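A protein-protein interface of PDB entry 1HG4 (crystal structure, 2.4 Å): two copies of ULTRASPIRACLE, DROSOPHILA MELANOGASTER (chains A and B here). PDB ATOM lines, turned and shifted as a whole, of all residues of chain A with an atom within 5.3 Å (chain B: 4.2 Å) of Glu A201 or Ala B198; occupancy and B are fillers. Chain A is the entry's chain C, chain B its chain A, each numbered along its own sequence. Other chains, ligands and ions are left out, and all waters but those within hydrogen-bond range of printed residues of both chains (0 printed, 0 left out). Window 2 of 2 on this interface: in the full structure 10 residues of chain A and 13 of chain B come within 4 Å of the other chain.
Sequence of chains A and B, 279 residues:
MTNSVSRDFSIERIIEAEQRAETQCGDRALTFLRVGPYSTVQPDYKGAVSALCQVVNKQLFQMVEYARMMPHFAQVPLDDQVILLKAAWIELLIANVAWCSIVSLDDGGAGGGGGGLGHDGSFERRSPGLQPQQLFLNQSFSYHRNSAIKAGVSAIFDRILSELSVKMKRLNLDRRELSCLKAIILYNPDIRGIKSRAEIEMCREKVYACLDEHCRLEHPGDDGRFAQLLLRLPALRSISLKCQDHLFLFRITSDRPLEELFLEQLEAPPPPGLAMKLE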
ATOM      1  N   PRO A 189      16.580   3.555   3.214  1.00  0.00           N
ATOM      2  CA  PRO A 189      16.128   4.607   4.129  1.00  0.00           C
ATOM      3  C   PRO A 189      16.416   6.045   3.714  1.00  0.00           C
ATOM      4  O   PRO A 189      15.929   6.980   4.353  1.00  0.00           O
ATOM      5  CB  PRO A 189      16.844   4.245   5.421  1.00  0.00           C
ATOM      6  CG  PRO A 189      18.195   3.830   4.904  1.00  0.00           C
ATOM      7  CD  PRO A 189      17.853   2.965   3.681  1.00  0.00           C
ATOM      8  N   SER A 196       9.601   6.014   8.326  1.00  0.00           N
ATOM      9  CA  SER A 196      10.319   5.063   9.154  1.00  0.00           C
ATOM     10  C   SER A 196      11.750   4.745   8.723  1.00  0.00           C
ATOM     11  O   SER A 196      12.087   3.583   8.478  1.00  0.00           O
ATOM     12  CB  SER A 196       9.508   3.774   9.227  1.00  0.00           C
ATOM     13  OG  SER A 196       8.151   4.079   9.496  1.00  0.00           O
ATOM     14  N   ARG A 197      12.595   5.771   8.653  1.00  0.00           N
ATOM     15  CA  ARG A 197      13.986   5.582   8.251  1.00  0.00           C
ATOM     16  C   ARG A 197      14.763   4.599   9.123  1.00  0.00           C
ATOM     17  O   ARG A 197      15.473   3.734   8.595  1.00  0.00           O
ATOM     18  CB  ARG A 197      14.740   6.915   8.236  1.00  0.00           C
ATOM     19  CG  ARG A 197      14.333   7.870   7.130  1.00  0.00           C
ATOM     20  CD  ARG A 197      15.223   9.119   7.124  1.00  0.00           C
ATOM     21  NE  ARG A 197      14.630  10.228   6.369  1.00  0.00           N
ATOM     22  CZ  ARG A 197      14.526  10.279   5.039  1.00  0.00           C
ATOM     23  NH1 ARG A 197      14.984   9.282   4.285  1.00  0.00           N
ATOM     24  NH2 ARG A 197      13.941  11.322   4.460  1.00  0.00           N
ATOM     25  N   ALA A 198      14.633   4.732  10.446  1.00  0.00           N
ATOM     26  CA  ALA A 198      15.354   3.858  11.370  1.00  0.00           C
ATOM     27  C   ALA A 198      15.030   2.388  11.151  1.00  0.00           C
ATOM     28  O   ALA A 198      15.935   1.564  11.027  1.00  0.00           O
ATOM     29  CB  ALA A 198      15.065   4.252  12.809  1.00  0.00           C
ATOM     30  N   GLU A 199      13.747   2.059  11.082  1.00  0.00           N
ATOM     31  CA  GLU A 199      13.327   0.682  10.871  1.00  0.00           C
ATOM     32  C   GLU A 199      13.841   0.141   9.537  1.00  0.00           C
ATOM     33  O   GLU A 199      14.284  -1.004   9.434  1.00  0.00           O
ATOM     34  CB  GLU A 199      11.800   0.589  10.903  1.00  0.00           C
ATOM     35  CG  GLU A 199      11.265  -0.806  10.579  1.00  0.00           C
ATOM     36  CD  GLU A 199      11.779  -1.868  11.548  1.00  0.00           C
ATOM     37  OE1 GLU A 199      11.341  -1.845  12.725  1.00  0.00           O
ATOM     38  OE2 GLU A 199      12.624  -2.711  11.141  1.00  0.00           O
ATOM     39  N   ILE A 200      13.770   0.971   8.508  1.00  0.00           N
ATOM     40  CA  ILE A 200      14.214   0.558   7.195  1.00  0.00           C
ATOM     41  C   ILE A 200      15.715   0.255   7.214  1.00  0.00           C
ATOM     42  O   ILE A 200      16.154  -0.774   6.677  1.00  0.00           O
ATOM     43  CB  ILE A 200      13.831   1.640   6.162  1.00  0.00           C
ATOM     44  CG1 ILE A 200      12.304   1.617   5.985  1.00  0.00           C
ATOM     45  CG2 ILE A 200      14.563   1.428   4.845  1.00  0.00           C
ATOM     46  CD1 ILE A 200      11.691   2.931   5.453  1.00  0.00           C
ATOM     47  N   GLU A 201      16.487   1.131   7.858  1.00  0.00           N
ATOM     48  CA  GLU A 201      17.931   0.951   7.986  1.00  0.00           C
ATOM     49  C   GLU A 201      18.234  -0.299   8.826  1.00  0.00           C
ATOM     50  O   GLU A 201      19.129  -1.096   8.530  1.00  0.00           O
ATOM     51  CB  GLU A 201      18.541   2.187   8.651  1.00  0.00           C
ATOM     52  CG  GLU A 201      20.016   2.065   8.990  1.00  0.00           C
ATOM     53  CD  GLU A 201      20.910   1.814   7.778  1.00  0.00           C
ATOM     54  OE1 GLU A 201      20.781   2.543   6.775  1.00  0.00           O
ATOM     55  OE2 GLU A 201      21.755   0.901   7.830  1.00  0.00           O
ATOM     56  N   MET A 202      17.460  -0.476   9.879  1.00  0.00           N
ATOM     57  CA  MET A 202      17.655  -1.617  10.752  1.00  0.00           C
ATOM     58  C   MET A 202      17.455  -2.886   9.924  1.00  0.00           C
ATOM     59  O   MET A 202      18.140  -3.888  10.123  1.00  0.00           O
ATOM     60  CB  MET A 202      16.660  -1.528  11.919  1.00  0.00           C
ATOM     61  CG  MET A 202      17.188  -1.925  13.301  1.00  0.00           C
ATOM     62  SD  MET A 202      18.651  -1.019  13.898  1.00  0.00           S
ATOM     63  CE  MET A 202      19.890  -2.330  13.706  1.00  0.00           C
ATOM     64  N   CYS A 203      16.530  -2.845   8.974  1.00  0.00           N
ATOM     65  CA  CYS A 203      16.283  -4.014   8.129  1.00  0.00           C
ATOM     66  C   CYS A 203      17.444  -4.310   7.196  1.00  0.00           C
ATOM     67  O   CYS A 203      17.856  -5.454   7.021  1.00  0.00           O
ATOM     68  CB  CYS A 203      15.012  -3.812   7.315  1.00  0.00           C
ATOM     69  SG  CYS A 203      13.549  -4.147   8.279  1.00  0.00           S
ATOM     70  N   ARG A 204      17.957  -3.253   6.590  1.00  0.00           N
ATOM     71  CA  ARG A 204      19.082  -3.349   5.679  1.00  0.00           C
ATOM     72  C   ARG A 204      20.319  -3.898   6.393  1.00  0.00           C
ATOM     73  O   ARG A 204      21.058  -4.731   5.854  1.00  0.00           O
ATOM     74  CB  ARG A 204      19.395  -1.966   5.105  1.00  0.00           C
ATOM     75  CG  ARG A 204      20.758  -1.876   4.437  1.00  0.00           C
ATOM     76  CD  ARG A 204      20.991  -0.514   3.789  1.00  0.00           C
ATOM     77  NE  ARG A 204      20.264  -0.372   2.531  1.00  0.00           N
ATOM     78  CZ  ARG A 204      20.418   0.639   1.682  1.00  0.00           C
ATOM     79  NH1 ARG A 204      21.277   1.614   1.941  1.00  0.00           N
ATOM     80  NH2 ARG A 204      19.705   0.680   0.569  1.00  0.00           N
ATOM     81  N   GLU A 205      20.543  -3.431   7.616  1.00  0.00           N
ATOM     82  CA  GLU A 205      21.706  -3.883   8.357  1.00  0.00           C
ATOM     83  C   GLU A 205      21.619  -5.358   8.719  1.00  0.00           C
ATOM     84  O   GLU A 205      22.632  -6.041   8.778  1.00  0.00           O
ATOM     85  CB  GLU A 205      21.913  -2.986   9.584  1.00  0.00           C
ATOM     86  CG  GLU A 205      22.397  -1.586   9.176  1.00  0.00           C
ATOM     87  CD  GLU A 205      22.633  -0.651  10.347  1.00  0.00           C
ATOM     88  OE1 GLU A 205      22.790  -1.126  11.487  1.00  0.00           O
ATOM     89  OE2 GLU A 205      22.678   0.570  10.134  1.00  0.00           O
ATOM     90  N   LYS A 206      20.415  -5.866   8.936  1.00  0.00           N
ATOM     91  CA  LYS A 206      20.268  -7.284   9.246  1.00  0.00           C
ATOM     92  C   LYS A 206      20.587  -8.113   8.006  1.00  0.00           C
ATOM     93  O   LYS A 206      21.057  -9.251   8.117  1.00  0.00           O
ATOM     94  CB  LYS A 206      18.855  -7.576   9.745  1.00  0.00           C
ATOM     95  CG  LYS A 206      18.542  -6.864  11.044  1.00  0.00           C
ATOM     96  CD  LYS A 206      17.166  -7.207  11.578  1.00  0.00           C
ATOM     97  CE  LYS A 206      16.933  -6.532  12.939  1.00  0.00           C
ATOM     98  NZ  LYS A 206      15.548  -6.750  13.449  1.00  0.00           N
ATOM     99  N   TYR A 208      22.820  -7.135   5.814  1.00  0.00           N
ATOM    100  CA  TYR A 208      24.282  -7.042   5.735  1.00  0.00           C
ATOM    101  C   TYR A 208      24.857  -8.199   6.552  1.00  0.00           C
ATOM    102  O   TYR A 208      25.749  -8.934   6.100  1.00  0.00           O
ATOM    103  CB  TYR A 208      24.778  -5.727   6.348  1.00  0.00           C
ATOM    104  CG  TYR A 208      24.675  -4.497   5.461  1.00  0.00           C
ATOM    105  CD1 TYR A 208      24.697  -4.600   4.073  1.00  0.00           C
ATOM    106  CD2 TYR A 208      24.576  -3.228   6.025  1.00  0.00           C
ATOM    107  CE1 TYR A 208      24.627  -3.465   3.273  1.00  0.00           C
ATOM    108  CE2 TYR A 208      24.497  -2.098   5.242  1.00  0.00           C
ATOM    109  CZ  TYR A 208      24.521  -2.213   3.867  1.00  0.00           C
ATOM    110  OH  TYR A 208      24.416  -1.073   3.099  1.00  0.00           O
ATOM    111  N   SER B 196      27.083  -1.083   9.553  1.00  0.00           N
ATOM    112  CA  SER B 196      25.987  -1.178  10.509  1.00  0.00           C
ATOM    113  C   SER B 196      25.932  -0.097  11.594  1.00  0.00           C
ATOM    114  O   SER B 196      25.937  -0.407  12.777  1.00  0.00           O
ATOM    115  CB  SER B 196      26.032  -2.554  11.157  1.00  0.00           C
ATOM    116  OG  SER B 196      26.221  -3.548  10.160  1.00  0.00           O
ATOM    117  N   ARG B 197      25.846   1.164  11.187  1.00  0.00           N
ATOM    118  CA  ARG B 197      25.783   2.274  12.131  1.00  0.00           C
ATOM    119  C   ARG B 197      24.626   2.185  13.109  1.00  0.00           C
ATOM    120  O   ARG B 197      24.821   2.376  14.304  1.00  0.00           O
ATOM    121  CB  ARG B 197      25.686   3.612  11.393  1.00  0.00           C
ATOM    122  CG  ARG B 197      26.943   4.021  10.644  1.00  0.00           C
ATOM    123  CD  ARG B 197      26.796   5.427  10.057  1.00  0.00           C
ATOM    124  NE  ARG B 197      27.803   5.701   9.030  1.00  0.00           N
ATOM    125  CZ  ARG B 197      29.096   5.932   9.264  1.00  0.00           C
ATOM    126  NH1 ARG B 197      29.575   5.936  10.505  1.00  0.00           N
ATOM    127  NH2 ARG B 197      29.919   6.146   8.244  1.00  0.00           N
ATOM    128  N   ALA B 198      23.424   1.899  12.606  1.00  0.00           N
ATOM    129  CA  ALA B 198      22.237   1.807  13.459  1.00  0.00           C
ATOM    130  C   ALA B 198      22.393   0.759  14.557  1.00  0.00           C
ATOM    131  O   ALA B 198      22.204   1.047  15.737  1.00  0.00           O
ATOM    132  CB  ALA B 198      20.999   1.503  12.609  1.00  0.00           C
ATOM    133  N   GLU B 199      22.725  -0.461  14.155  1.00  0.00           N
ATOM    134  CA  GLU B 199      22.932  -1.545  15.109  1.00  0.00           C
ATOM    135  C   GLU B 199      23.960  -1.171  16.177  1.00  0.00           C
ATOM    136  O   GLU B 199      23.757  -1.441  17.357  1.00  0.00           O
ATOM    137  CB  GLU B 199      23.393  -2.804  14.378  1.00  0.00           C
ATOM    138  CG  GLU B 199      24.071  -3.830  15.279  1.00  0.00           C
ATOM    139  CD  GLU B 199      23.100  -4.615  16.152  1.00  0.00           C
ATOM    140  OE1 GLU B 199      21.936  -4.186  16.302  1.00  0.00           O
ATOM    141  OE2 GLU B 199      23.516  -5.662  16.698  1.00  0.00           O
ATOM    142  N   ILE B 200      25.055  -0.539  15.769  1.00  0.00           N
ATOM    143  CA  ILE B 200      26.101  -0.154  16.711  1.00  0.00           C
ATOM    144  C   ILE B 200      25.643   0.953  17.690  1.00  0.00           C
ATOM    145  O   ILE B 200      25.909   0.883  18.902  1.00  0.00           O
ATOM    146  CB  ILE B 200      27.376   0.276  15.932  1.00  0.00           C
ATOM    147  CG1 ILE B 200      27.807  -0.856  14.995  1.00  0.00           C
ATOM    148  CG2 ILE B 200      28.506   0.559  16.878  1.00  0.00           C
ATOM    149  CD1 ILE B 200      29.025  -0.530  14.160  1.00  0.00           C
ATOM    150  N   GLU B 201      24.945   1.959  17.168  1.00  0.00           N
ATOM    151  CA  GLU B 201      24.443   3.057  17.990  1.00  0.00           C
ATOM    152  C   GLU B 201      23.471   2.521  19.024  1.00  0.00           C
ATOM    153  O   GLU B 201      23.366   3.040  20.134  1.00  0.00           O
ATOM    154  CB  GLU B 201      23.724   4.097  17.123  1.00  0.00           C
ATOM    155  CG  GLU B 201      22.897   5.116  17.911  1.00  0.00           C
ATOM    156  CD  GLU B 201      23.732   6.082  18.779  1.00  0.00           C
ATOM    157  OE1 GLU B 201      24.974   6.107  18.661  1.00  0.00           O
ATOM    158  OE2 GLU B 201      23.128   6.842  19.573  1.00  0.00           O
ATOM    159  N   MET B 202      22.757   1.473  18.647  1.00  0.00           N
ATOM    160  CA  MET B 202      21.775   0.865  19.522  1.00  0.00           C
ATOM    161  C   MET B 202      22.485   0.208  20.723  1.00  0.00           C
ATOM    162  O   MET B 202      22.106   0.426  21.879  1.00  0.00           O
ATOM    163  CB  MET B 202      20.939  -0.134  18.707  1.00  0.00           C
ATOM    164  CG  MET B 202      19.469  -0.170  19.089  1.00  0.00           C
ATOM    165  SD  MET B 202      18.741   1.491  19.370  1.00  0.00           S
ATOM    166  CE  MET B 202      18.816   1.557  21.155  1.00  0.00           C
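The backbone carbonyl oxygen (O) of Ser B196 sits close to the side-chain carboxylate (OE1) of Glu A205, at 3.5 Å. The backbone NH of Ala B198 is in hydrogen-bond range of the side-chain carboxylate of Glu A205 (2.9 Å). The backbone NH of Glu B199 sits at hydrogen-bond distance from the side-chain carboxylate of Glu A205 (2.8 Å). The backbone NH (N) of Arg B197 lies within hydrogen-bond range of the side-chain carboxylate (OE2) of Glu A205.
Among the printed residues, merely in contact across the chains: Glu A201 with Ala B198, Met A202 with Ala B198 and Met A202 with Glu B199.
OE2 of Glu A205 lies close to OE2 of Glu A201.
Glu A201 touches Ala B198, but with the chains exchanged Ala A198 does not touch Glu B201 (9.4 Å). Met A202 touches Ala B198, but with the chains exchanged Ala A198 does not touch Met B202 (8.0 Å). Met A202 touches Glu B199, but with the chains exchanged Glu A199 does not touch Met B202 (9.7 Å).
Of the 7 printed residues of chain B, 4 touch a printed residue of chain A. Hydrophobic or aromatic side chains of chain B that line the printed part of chain A: Ala B198. Hydrophobic or aromatic side chains of chain A within 4 Å of the printed part of chain B: Met A202. Along chain A the printed residues that touch a printed residue of chain B span positions 201 to 205. Among the printed residues, no Asp or Glu carboxylate lies within 4 Å of a Lys or Arg side-chain nitrogen of the other chain.
Arg A197 touches none of the printed residues of chain B. Lys A206 touches none of the printed residues of chain B. Of the printed residues of chain A, Ser B196 touches Glu A205. Of the printed residues of chain A, Arg B197 touches Glu A205. Printed residues of chain A within 4 Å of Ala B198: Glu A201, Met A202 and Glu A205. Printed residues of chain A within 4 Å of Glu B199: Met A202 (3.4 Å) and Glu A205 (2.8 Å). The nearest printed residue of chain B that does not touch Glu A201 is Arg B197 (5.3 Å).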
